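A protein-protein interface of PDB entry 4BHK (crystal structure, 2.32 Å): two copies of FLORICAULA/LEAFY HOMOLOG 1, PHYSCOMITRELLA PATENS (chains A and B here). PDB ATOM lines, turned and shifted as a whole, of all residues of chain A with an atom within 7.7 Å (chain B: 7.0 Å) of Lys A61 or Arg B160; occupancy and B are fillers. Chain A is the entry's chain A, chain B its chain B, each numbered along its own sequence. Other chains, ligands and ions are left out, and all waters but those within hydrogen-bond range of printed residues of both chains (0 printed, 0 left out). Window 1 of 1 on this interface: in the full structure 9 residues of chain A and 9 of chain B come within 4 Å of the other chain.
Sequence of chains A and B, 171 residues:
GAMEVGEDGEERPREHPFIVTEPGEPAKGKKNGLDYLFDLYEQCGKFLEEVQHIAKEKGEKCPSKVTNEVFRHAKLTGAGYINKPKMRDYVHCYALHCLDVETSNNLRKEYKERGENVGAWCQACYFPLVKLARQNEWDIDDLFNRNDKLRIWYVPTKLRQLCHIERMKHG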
ATOM      1  N   VAL A  51     -13.356   0.991 -12.434  1.00  0.00           N
ATOM      2  CA  VAL A  51     -12.082   0.888 -11.724  1.00  0.00           C
ATOM      3  C   VAL A  51     -11.289  -0.326 -12.257  1.00  0.00           C
ATOM      4  O   VAL A  51     -10.104  -0.174 -12.560  1.00  0.00           O
ATOM      5  CB  VAL A  51     -12.273   0.862 -10.187  1.00  0.00           C
ATOM      6  CG1 VAL A  51     -10.957   0.536  -9.454  1.00  0.00           C
ATOM      7  CG2 VAL A  51     -12.852   2.180  -9.693  1.00  0.00           C
ATOM      8  N   GLN A  52     -11.970  -1.494 -12.433  1.00  0.00           N
ATOM      9  CA  GLN A  52     -11.385  -2.760 -12.942  1.00  0.00           C
ATOM     10  C   GLN A  52     -10.853  -2.591 -14.364  1.00  0.00           C
ATOM     11  O   GLN A  52      -9.696  -2.924 -14.613  1.00  0.00           O
ATOM     12  CB  GLN A  52     -12.409  -3.908 -12.900  1.00  0.00           C
ATOM     13  CG  GLN A  52     -12.653  -4.475 -11.505  1.00  0.00           C
ATOM     14  CD  GLN A  52     -13.727  -5.540 -11.463  1.00  0.00           C
ATOM     15  OE1 GLN A  52     -14.709  -5.512 -12.215  1.00  0.00           O
ATOM     16  NE2 GLN A  52     -13.583  -6.498 -10.555  1.00  0.00           N
ATOM     17  N   ILE A  54     -10.127   0.256 -16.005  1.00  0.00           N
ATOM     18  CA  ILE A  54      -9.044   1.253 -15.990  1.00  0.00           C
ATOM     19  C   ILE A  54      -7.715   0.616 -15.579  1.00  0.00           C
ATOM     20  O   ILE A  54      -6.724   0.809 -16.282  1.00  0.00           O
ATOM     21  CB  ILE A  54      -9.408   2.533 -15.180  1.00  0.00           C
ATOM     22  CG1 ILE A  54     -10.505   3.360 -15.921  1.00  0.00           C
ATOM     23  CG2 ILE A  54      -8.176   3.410 -14.907  1.00  0.00           C
ATOM     24  CD1 ILE A  54     -11.333   4.374 -14.994  1.00  0.00           C
ATOM     25  N   ALA A  55      -7.719  -0.178 -14.477  1.00  0.00           N
ATOM     26  CA  ALA A  55      -6.557  -0.881 -13.923  1.00  0.00           C
ATOM     27  C   ALA A  55      -5.967  -1.830 -14.942  1.00  0.00           C
ATOM     28  O   ALA A  55      -4.747  -1.838 -15.107  1.00  0.00           O
ATOM     29  CB  ALA A  55      -6.946  -1.639 -12.666  1.00  0.00           C
ATOM     30  N   LYS A  56      -6.825  -2.601 -15.650  1.00  0.00           N
ATOM     31  CA  LYS A  56      -6.407  -3.547 -16.685  1.00  0.00           C
ATOM     32  C   LYS A  56      -5.637  -2.820 -17.788  1.00  0.00           C
ATOM     33  O   LYS A  56      -4.577  -3.303 -18.193  1.00  0.00           O
ATOM     34  CB  LYS A  56      -7.601  -4.334 -17.248  1.00  0.00           C
ATOM     35  CG  LYS A  56      -8.140  -5.399 -16.291  1.00  0.00           C
ATOM     36  CD  LYS A  56      -8.815  -6.538 -17.036  1.00  0.00           C
ATOM     37  CE  LYS A  56      -9.159  -7.680 -16.111  1.00  0.00           C
ATOM     38  NZ  LYS A  56      -9.687  -8.861 -16.849  1.00  0.00           N
ATOM     39  N   LYS A  58      -4.047   0.264 -17.455  1.00  0.00           N
ATOM     40  CA  LYS A  58      -2.841   0.843 -16.867  1.00  0.00           C
ATOM     41  C   LYS A  58      -1.782  -0.235 -16.497  1.00  0.00           C
ATOM     42  O   LYS A  58      -0.614   0.106 -16.269  1.00  0.00           O
ATOM     43  CB  LYS A  58      -3.195   1.700 -15.634  1.00  0.00           C
ATOM     44  CG  LYS A  58      -4.180   2.849 -15.891  1.00  0.00           C
ATOM     45  CD  LYS A  58      -3.620   4.177 -15.399  1.00  0.00           C
ATOM     46  CE  LYS A  58      -4.616   4.957 -14.579  1.00  0.00           C
ATOM     47  NZ  LYS A  58      -4.626   4.523 -13.160  1.00  0.00           N
ATOM     48  N   GLY A  59      -2.196  -1.508 -16.448  1.00  0.00           N
ATOM     49  CA  GLY A  59      -1.337  -2.618 -16.050  1.00  0.00           C
ATOM     50  C   GLY A  59      -1.103  -2.607 -14.550  1.00  0.00           C
ATOM     51  O   GLY A  59       0.006  -2.887 -14.083  1.00  0.00           O
ATOM     52  N   GLU A  60      -2.148  -2.239 -13.791  1.00  0.00           N
ATOM     53  CA  GLU A  60      -2.129  -2.122 -12.336  1.00  0.00           C
ATOM     54  C   GLU A  60      -2.971  -3.217 -11.669  1.00  0.00           C
ATOM     55  O   GLU A  60      -3.728  -3.915 -12.354  1.00  0.00           O
ATOM     56  CB  GLU A  60      -2.627  -0.728 -11.910  1.00  0.00           C
ATOM     57  CG  GLU A  60      -1.747   0.421 -12.385  1.00  0.00           C
ATOM     58  CD  GLU A  60      -2.051   1.797 -11.821  1.00  0.00           C
ATOM     59  OE1 GLU A  60      -3.219   2.060 -11.453  1.00  0.00           O
ATOM     60  OE2 GLU A  60      -1.119   2.634 -11.785  1.00  0.00           O
ATOM     61  N   LYS A  61      -2.830  -3.372 -10.332  1.00  0.00           N
ATOM     62  CA  LYS A  61      -3.585  -4.358  -9.538  1.00  0.00           C
ATOM     63  C   LYS A  61      -5.096  -4.112  -9.721  1.00  0.00           C
ATOM     64  O   LYS A  61      -5.569  -2.974  -9.657  1.00  0.00           O
ATOM     65  CB  LYS A  61      -3.181  -4.302  -8.057  1.00  0.00           C
ATOM     66  CG  LYS A  61      -3.643  -5.502  -7.226  1.00  0.00           C
ATOM     67  CD  LYS A  61      -2.776  -5.743  -5.961  1.00  0.00           C
ATOM     68  CE  LYS A  61      -3.079  -4.828  -4.791  1.00  0.00           C
ATOM     69  NZ  LYS A  61      -2.425  -5.287  -3.539  1.00  0.00           N
ATOM     70  N   CYS A  62      -5.818  -5.179 -10.027  1.00  0.00           N
ATOM     71  CA  CYS A  62      -7.234  -5.116 -10.309  1.00  0.00           C
ATOM     72  C   CYS A  62      -8.046  -5.638  -9.117  1.00  0.00           C
ATOM     73  O   CYS A  62      -7.853  -6.786  -8.701  1.00  0.00           O
ATOM     74  CB  CYS A  62      -7.536  -5.892 -11.583  1.00  0.00           C
ATOM     75  SG  CYS A  62      -9.251  -5.778 -12.119  1.00  0.00           S
ATOM     76  N   PRO A  63      -8.937  -4.810  -8.533  1.00  0.00           N
ATOM     77  CA  PRO A  63      -9.714  -5.289  -7.388  1.00  0.00           C
ATOM     78  C   PRO A  63     -10.811  -6.269  -7.808  1.00  0.00           C
ATOM     79  O   PRO A  63     -11.384  -6.109  -8.882  1.00  0.00           O
ATOM     80  CB  PRO A  63     -10.271  -4.001  -6.789  1.00  0.00           C
ATOM     81  CG  PRO A  63     -10.383  -3.065  -7.950  1.00  0.00           C
ATOM     82  CD  PRO A  63      -9.286  -3.414  -8.888  1.00  0.00           C
ATOM     83  N   SER A  64     -11.084  -7.289  -6.978  1.00  0.00           N
ATOM     84  CA  SER A  64     -12.145  -8.273  -7.261  1.00  0.00           C
ATOM     85  C   SER A  64     -13.438  -7.913  -6.479  1.00  0.00           C
ATOM     86  O   SER A  64     -14.507  -8.467  -6.750  1.00  0.00           O
ATOM     87  CB  SER A  64     -11.684  -9.681  -6.882  1.00  0.00           C
ATOM     88  OG  SER A  64     -11.572  -9.802  -5.473  1.00  0.00           O
ATOM     89  N   TYR B 126      11.927 -13.374 -15.016  1.00  0.00           N
ATOM     90  CA  TYR B 126      10.846 -12.502 -15.513  1.00  0.00           C
ATOM     91  C   TYR B 126      10.583 -12.714 -17.010  1.00  0.00           C
ATOM     92  O   TYR B 126       9.432 -12.784 -17.435  1.00  0.00           O
ATOM     93  CB  TYR B 126      11.232 -11.020 -15.296  1.00  0.00           C
ATOM     94  CG  TYR B 126      11.201 -10.551 -13.859  1.00  0.00           C
ATOM     95  CD1 TYR B 126       9.997 -10.339 -13.202  1.00  0.00           C
ATOM     96  CD2 TYR B 126      12.382 -10.307 -13.158  1.00  0.00           C
ATOM     97  CE1 TYR B 126       9.962  -9.924 -11.875  1.00  0.00           C
ATOM     98  CE2 TYR B 126      12.360  -9.889 -11.831  1.00  0.00           C
ATOM     99  CZ  TYR B 126      11.146  -9.711 -11.188  1.00  0.00           C
ATOM    100  OH  TYR B 126      11.101  -9.274  -9.888  1.00  0.00           O
ATOM    101  N   TRP B 138      -1.909 -11.502 -22.549  1.00  0.00           N
ATOM    102  CA  TRP B 138      -1.283 -10.584 -21.585  1.00  0.00           C
ATOM    103  C   TRP B 138      -1.874 -10.589 -20.164  1.00  0.00           C
ATOM    104  O   TRP B 138      -1.547  -9.724 -19.349  1.00  0.00           O
ATOM    105  CB  TRP B 138      -1.118  -9.179 -22.176  1.00  0.00           C
ATOM    106  CG  TRP B 138      -0.135  -9.142 -23.314  1.00  0.00           C
ATOM    107  CD1 TRP B 138      -0.425  -9.111 -24.645  1.00  0.00           C
ATOM    108  CD2 TRP B 138       1.300  -9.191 -23.215  1.00  0.00           C
ATOM    109  NE1 TRP B 138       0.737  -9.093 -25.383  1.00  0.00           N
ATOM    110  CE2 TRP B 138       1.811  -9.137 -24.530  1.00  0.00           C
ATOM    111  CE3 TRP B 138       2.204  -9.266 -22.136  1.00  0.00           C
ATOM    112  CZ2 TRP B 138       3.187  -9.145 -24.801  1.00  0.00           C
ATOM    113  CZ3 TRP B 138       3.566  -9.292 -22.405  1.00  0.00           C
ATOM    114  CH2 TRP B 138       4.045  -9.240 -23.724  1.00  0.00           C
ATOM    115  N   ILE B 140      -1.549 -11.876 -16.905  1.00  0.00           N
ATOM    116  CA  ILE B 140      -0.655 -12.495 -15.945  1.00  0.00           C
ATOM    117  C   ILE B 140      -1.415 -12.933 -14.673  1.00  0.00           C
ATOM    118  O   ILE B 140      -1.101 -13.970 -14.088  1.00  0.00           O
ATOM    119  CB  ILE B 140       0.626 -11.630 -15.701  1.00  0.00           C
ATOM    120  CG1 ILE B 140       1.677 -12.359 -14.828  1.00  0.00           C
ATOM    121  CG2 ILE B 140       0.298 -10.236 -15.153  1.00  0.00           C
ATOM    122  CD1 ILE B 140       2.161 -13.796 -15.348  1.00  0.00           C
ATOM    123  N   ASP B 141      -2.455 -12.180 -14.310  1.00  0.00           N
ATOM    124  CA  ASP B 141      -3.311 -12.473 -13.171  1.00  0.00           C
ATOM    125  C   ASP B 141      -4.076 -13.770 -13.347  1.00  0.00           C
ATOM    126  O   ASP B 141      -4.056 -14.600 -12.439  1.00  0.00           O
ATOM    127  CB  ASP B 141      -4.214 -11.280 -12.839  1.00  0.00           C
ATOM    128  CG  ASP B 141      -3.467 -10.222 -12.047  1.00  0.00           C
ATOM    129  OD1 ASP B 141      -2.539  -9.583 -12.617  1.00  0.00           O
ATOM    130  OD2 ASP B 141      -3.743 -10.086 -10.836  1.00  0.00           O
ATOM    131  N   TYR B 154       0.232 -13.715  -4.540  1.00  0.00           N
ATOM    132  CA  TYR B 154      -0.096 -12.441  -5.184  1.00  0.00           C
ATOM    133  C   TYR B 154       0.858 -12.245  -6.349  1.00  0.00           C
ATOM    134  O   TYR B 154       2.044 -12.609  -6.257  1.00  0.00           O
ATOM    135  CB  TYR B 154       0.070 -11.282  -4.200  1.00  0.00           C
ATOM    136  CG  TYR B 154      -1.016 -11.171  -3.152  1.00  0.00           C
ATOM    137  CD1 TYR B 154      -2.254 -10.606  -3.457  1.00  0.00           C
ATOM    138  CD2 TYR B 154      -0.773 -11.532  -1.830  1.00  0.00           C
ATOM    139  CE1 TYR B 154      -3.242 -10.463  -2.483  1.00  0.00           C
ATOM    140  CE2 TYR B 154      -1.743 -11.362  -0.843  1.00  0.00           C
ATOM    141  CZ  TYR B 154      -2.987 -10.853  -1.179  1.00  0.00           C
ATOM    142  OH  TYR B 154      -3.944 -10.705  -0.208  1.00  0.00           O
ATOM    143  N   VAL B 155       0.341 -11.691  -7.454  1.00  0.00           N
ATOM    144  CA  VAL B 155       1.155 -11.392  -8.633  1.00  0.00           C
ATOM    145  C   VAL B 155       2.164 -10.284  -8.230  1.00  0.00           C
ATOM    146  O   VAL B 155       1.744  -9.235  -7.719  1.00  0.00           O
ATOM    147  CB  VAL B 155       0.300 -10.992  -9.883  1.00  0.00           C
ATOM    148  CG1 VAL B 155       1.190 -10.616 -11.051  1.00  0.00           C
ATOM    149  CG2 VAL B 155      -0.648 -12.119 -10.290  1.00  0.00           C
ATOM    150  N   PRO B 156       3.487 -10.519  -8.396  1.00  0.00           N
ATOM    151  CA  PRO B 156       4.458  -9.459  -8.041  1.00  0.00           C
ATOM    152  C   PRO B 156       4.316  -8.217  -8.908  1.00  0.00           C
ATOM    153  O   PRO B 156       4.209  -8.331 -10.133  1.00  0.00           O
ATOM    154  CB  PRO B 156       5.833 -10.117  -8.238  1.00  0.00           C
ATOM    155  CG  PRO B 156       5.581 -11.523  -8.624  1.00  0.00           C
ATOM    156  CD  PRO B 156       4.147 -11.709  -8.977  1.00  0.00           C
ATOM    157  N   THR B 157       4.323  -7.035  -8.269  1.00  0.00           N
ATOM    158  CA  THR B 157       4.228  -5.733  -8.929  1.00  0.00           C
ATOM    159  C   THR B 157       5.159  -5.597 -10.138  1.00  0.00           C
ATOM    160  O   THR B 157       4.685  -5.212 -11.222  1.00  0.00           O
ATOM    161  CB  THR B 157       4.504  -4.613  -7.920  1.00  0.00           C
ATOM    162  OG1 THR B 157       3.644  -4.788  -6.793  1.00  0.00           O
ATOM    163  CG2 THR B 157       4.342  -3.202  -8.531  1.00  0.00           C
ATOM    164  N   LYS B 158       6.465  -5.910  -9.954  1.00  0.00           N
ATOM    165  CA  LYS B 158       7.482  -5.830 -11.005  1.00  0.00           C
ATOM    166  C   LYS B 158       7.130  -6.667 -12.251  1.00  0.00           C
ATOM    167  O   LYS B 158       7.388  -6.237 -13.374  1.00  0.00           O
ATOM    168  CB  LYS B 158       8.873  -6.186 -10.463  1.00  0.00           C
ATOM    169  CG  LYS B 158      10.028  -5.656 -11.309  1.00  0.00           C
ATOM    170  CD  LYS B 158      11.187  -5.138 -10.445  1.00  0.00           C
ATOM    171  CE  LYS B 158      12.286  -6.157 -10.222  1.00  0.00           C
ATOM    172  NZ  LYS B 158      12.700  -6.229  -8.793  1.00  0.00           N
ATOM    173  N   LEU B 159       6.513  -7.834 -12.053  1.00  0.00           N
ATOM    174  CA  LEU B 159       6.127  -8.680 -13.178  1.00  0.00           C
ATOM    175  C   LEU B 159       4.951  -8.067 -13.967  1.00  0.00           C
ATOM    176  O   LEU B 159       4.990  -8.053 -15.203  1.00  0.00           O
ATOM    177  CB  LEU B 159       5.817 -10.109 -12.703  1.00  0.00           C
ATOM    178  CG  LEU B 159       5.365 -11.103 -13.770  1.00  0.00           C
ATOM    179  CD1 LEU B 159       6.449 -11.312 -14.832  1.00  0.00           C
ATOM    180  CD2 LEU B 159       4.940 -12.423 -13.121  1.00  0.00           C
ATOM    181  N   ARG B 160       3.945  -7.555 -13.267  1.00  0.00           N
ATOM    182  CA  ARG B 160       2.816  -6.914 -13.932  1.00  0.00           C
ATOM    183  C   ARG B 160       3.279  -5.674 -14.729  1.00  0.00           C
ATOM    184  O   ARG B 160       2.882  -5.532 -15.873  1.00  0.00           O
ATOM    185  CB  ARG B 160       1.654  -6.602 -12.956  1.00  0.00           C
ATOM    186  CG  ARG B 160       0.284  -6.449 -13.660  1.00  0.00           C
ATOM    187  CD  ARG B 160      -0.936  -6.616 -12.737  1.00  0.00           C
ATOM    188  NE  ARG B 160      -0.624  -6.251 -11.357  1.00  0.00           N
ATOM    189  CZ  ARG B 160      -0.922  -6.977 -10.293  1.00  0.00           C
ATOM    190  NH1 ARG B 160      -1.625  -8.097 -10.419  1.00  0.00           N
ATOM    191  NH2 ARG B 160      -0.556  -6.572  -9.087  1.00  0.00           N
ATOM    192  N   GLN B 161       4.194  -4.860 -14.161  1.00  0.00           N
ATOM    193  CA  GLN B 161       4.752  -3.665 -14.807  1.00  0.00           C
ATOM    194  C   GLN B 161       5.560  -4.036 -16.033  1.00  0.00           C
ATOM    195  O   GLN B 161       5.375  -3.402 -17.074  1.00  0.00           O
ATOM    196  CB  GLN B 161       5.636  -2.866 -13.844  1.00  0.00           C
ATOM    197  CG  GLN B 161       4.900  -2.199 -12.695  1.00  0.00           C
ATOM    198  CD  GLN B 161       5.837  -1.389 -11.835  1.00  0.00           C
ATOM    199  OE1 GLN B 161       6.992  -1.770 -11.581  1.00  0.00           O
ATOM    200  NE2 GLN B 161       5.343  -0.271 -11.327  1.00  0.00           N
ATOM    201  N   LEU B 162       6.450  -5.068 -15.921  1.00  0.00           N
ATOM    202  CA  LEU B 162       7.268  -5.563 -17.035  1.00  0.00           C
ATOM    203  C   LEU B 162       6.387  -6.112 -18.153  1.00  0.00           C
ATOM    204  O   LEU B 162       6.720  -5.896 -19.315  1.00  0.00           O
ATOM    205  CB  LEU B 162       8.292  -6.639 -16.586  1.00  0.00           C
ATOM    206  CG  LEU B 162       9.254  -7.218 -17.681  1.00  0.00           C
ATOM    207  CD1 LEU B 162      10.201  -6.165 -18.248  1.00  0.00           C
ATOM    208  CD2 LEU B 162      10.091  -8.319 -17.148  1.00  0.00           C
ATOM    209  N   CYS B 163       5.283  -6.822 -17.813  1.00  0.00           N
ATOM    210  CA  CYS B 163       4.351  -7.392 -18.794  1.00  0.00           C
ATOM    211  C   CYS B 163       3.655  -6.309 -19.588  1.00  0.00           C
ATOM    212  O   CYS B 163       3.517  -6.451 -20.799  1.00  0.00           O
ATOM    213  CB  CYS B 163       3.347  -8.347 -18.147  1.00  0.00           C
ATOM    214  SG  CYS B 163       4.041  -9.969 -17.718  1.00  0.00           S
ATOM    215  N   HIS B 164       3.259  -5.216 -18.911  1.00  0.00           N
ATOM    216  CA  HIS B 164       2.577  -4.080 -19.504  1.00  0.00           C
ATOM    217  C   HIS B 164       3.466  -3.338 -20.494  1.00  0.00           C
ATOM    218  O   HIS B 164       3.024  -3.084 -21.601  1.00  0.00           O
ATOM    219  CB  HIS B 164       2.019  -3.149 -18.411  1.00  0.00           C
ATOM    220  CG  HIS B 164       1.367  -1.896 -18.912  1.00  0.00           C
ATOM    221  ND1 HIS B 164       0.377  -1.927 -19.874  1.00  0.00           N
ATOM    222  CD2 HIS B 164       1.515  -0.622 -18.493  1.00  0.00           C
ATOM    223  CE1 HIS B 164      -0.018  -0.676 -20.037  1.00  0.00           C
ATOM    224  NE2 HIS B 164       0.633   0.147 -19.230  1.00  0.00           N
ATOM    225  N   ILE B 165       4.720  -3.034 -20.112  1.00  0.00           N
ATOM    226  CA  ILE B 165       5.685  -2.344 -20.970  1.00  0.00           C
ATOM    227  C   ILE B 165       6.054  -3.183 -22.196  1.00  0.00           C
ATOM    228  O   ILE B 165       6.131  -2.642 -23.283  1.00  0.00           O
ATOM    229  CB  ILE B 165       6.918  -1.770 -20.207  1.00  0.00           C
ATOM    230  CG1 ILE B 165       7.883  -2.851 -19.694  1.00  0.00           C
ATOM    231  CG2 ILE B 165       6.494  -0.862 -19.064  1.00  0.00           C
ATOM    232  CD1 ILE B 165       9.141  -3.073 -20.588  1.00  0.00           C
ATOM    233  N   ARG B 167       4.231  -5.411 -23.742  1.00  0.00           N
ATOM    234  CA  ARG B 167       3.028  -5.424 -24.577  1.00  0.00           C
ATOM    235  C   ARG B 167       3.002  -4.161 -25.455  1.00  0.00           C
ATOM    236  O   ARG B 167       2.567  -4.221 -26.603  1.00  0.00           O
ATOM    237  CB  ARG B 167       1.769  -5.520 -23.689  1.00  0.00           C
ATOM    238  CG  ARG B 167       0.450  -5.195 -24.409  1.00  0.00           C
ATOM    239  CD  ARG B 167      -0.801  -5.693 -23.702  1.00  0.00           C
ATOM    240  NE  ARG B 167      -0.906  -5.300 -22.291  1.00  0.00           N
ATOM    241  CZ  ARG B 167      -1.583  -4.243 -21.851  1.00  0.00           C
ATOM    242  NH1 ARG B 167      -2.192  -3.431 -22.707  1.00  0.00           N
ATOM    243  NH2 ARG B 167      -1.653  -3.990 -20.551  1.00  0.00           N
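Of chain B, only Arg B160 (3.6 Å) comes within 4 Å of Lys A61. Arg B160 touches three residues of chain A. Of the printed residues of chain A, Arg B167 touches Lys A56. Of the printed residues of chain B, Lys A56 touches Arg B167 (3.8 Å). Of the printed residues of chain A, His B164 touches Lys A58. Ser A64 touches none of the printed residues of chain B. The nearest printed residue of chain B that does not touch Gly A59 is His B164 (4.003 Å).
The backbone carbonyl oxygen of Lys A58 lies close to a ring nitrogen (NE2) of His B164 (3.2 Å).
Printed residues of chain B that touch a printed residue of chain A: Arg B160, His B164 and Arg B167. Hydrophobic or aromatic side chains of chain B that line the printed part of chain A: His B164.
The side-chain carboxylate of Asp B141 is in salt-bridge range of the guanidinium group of Arg B160, at 2.8 Å. The side-chain carboxylate (OE1) of Glu A60 lies within salt-bridge range of the side-chain amino group (NZ) of Lys A58, 3.3 Å away. N of Glu A60 is in hydrogen-bond range of O of Ala A55 (2.9 Å). A ring nitrogen (ND1) of His B164 is in hydrogen-bond range of the guanidinium group (NH2) of Arg B167 (3.0 Å).
Among the printed residues, pairs that only touch across the chains: Gly A59 with Arg B160, Lys A61 with Arg B160, Lys A56 with Arg B167 and Glu A60 with Arg B160.
No position is printed for both chains. Of the 5 pairs that touch across the chains among the printed residues, none has its exchanged pair printed and touching as well.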
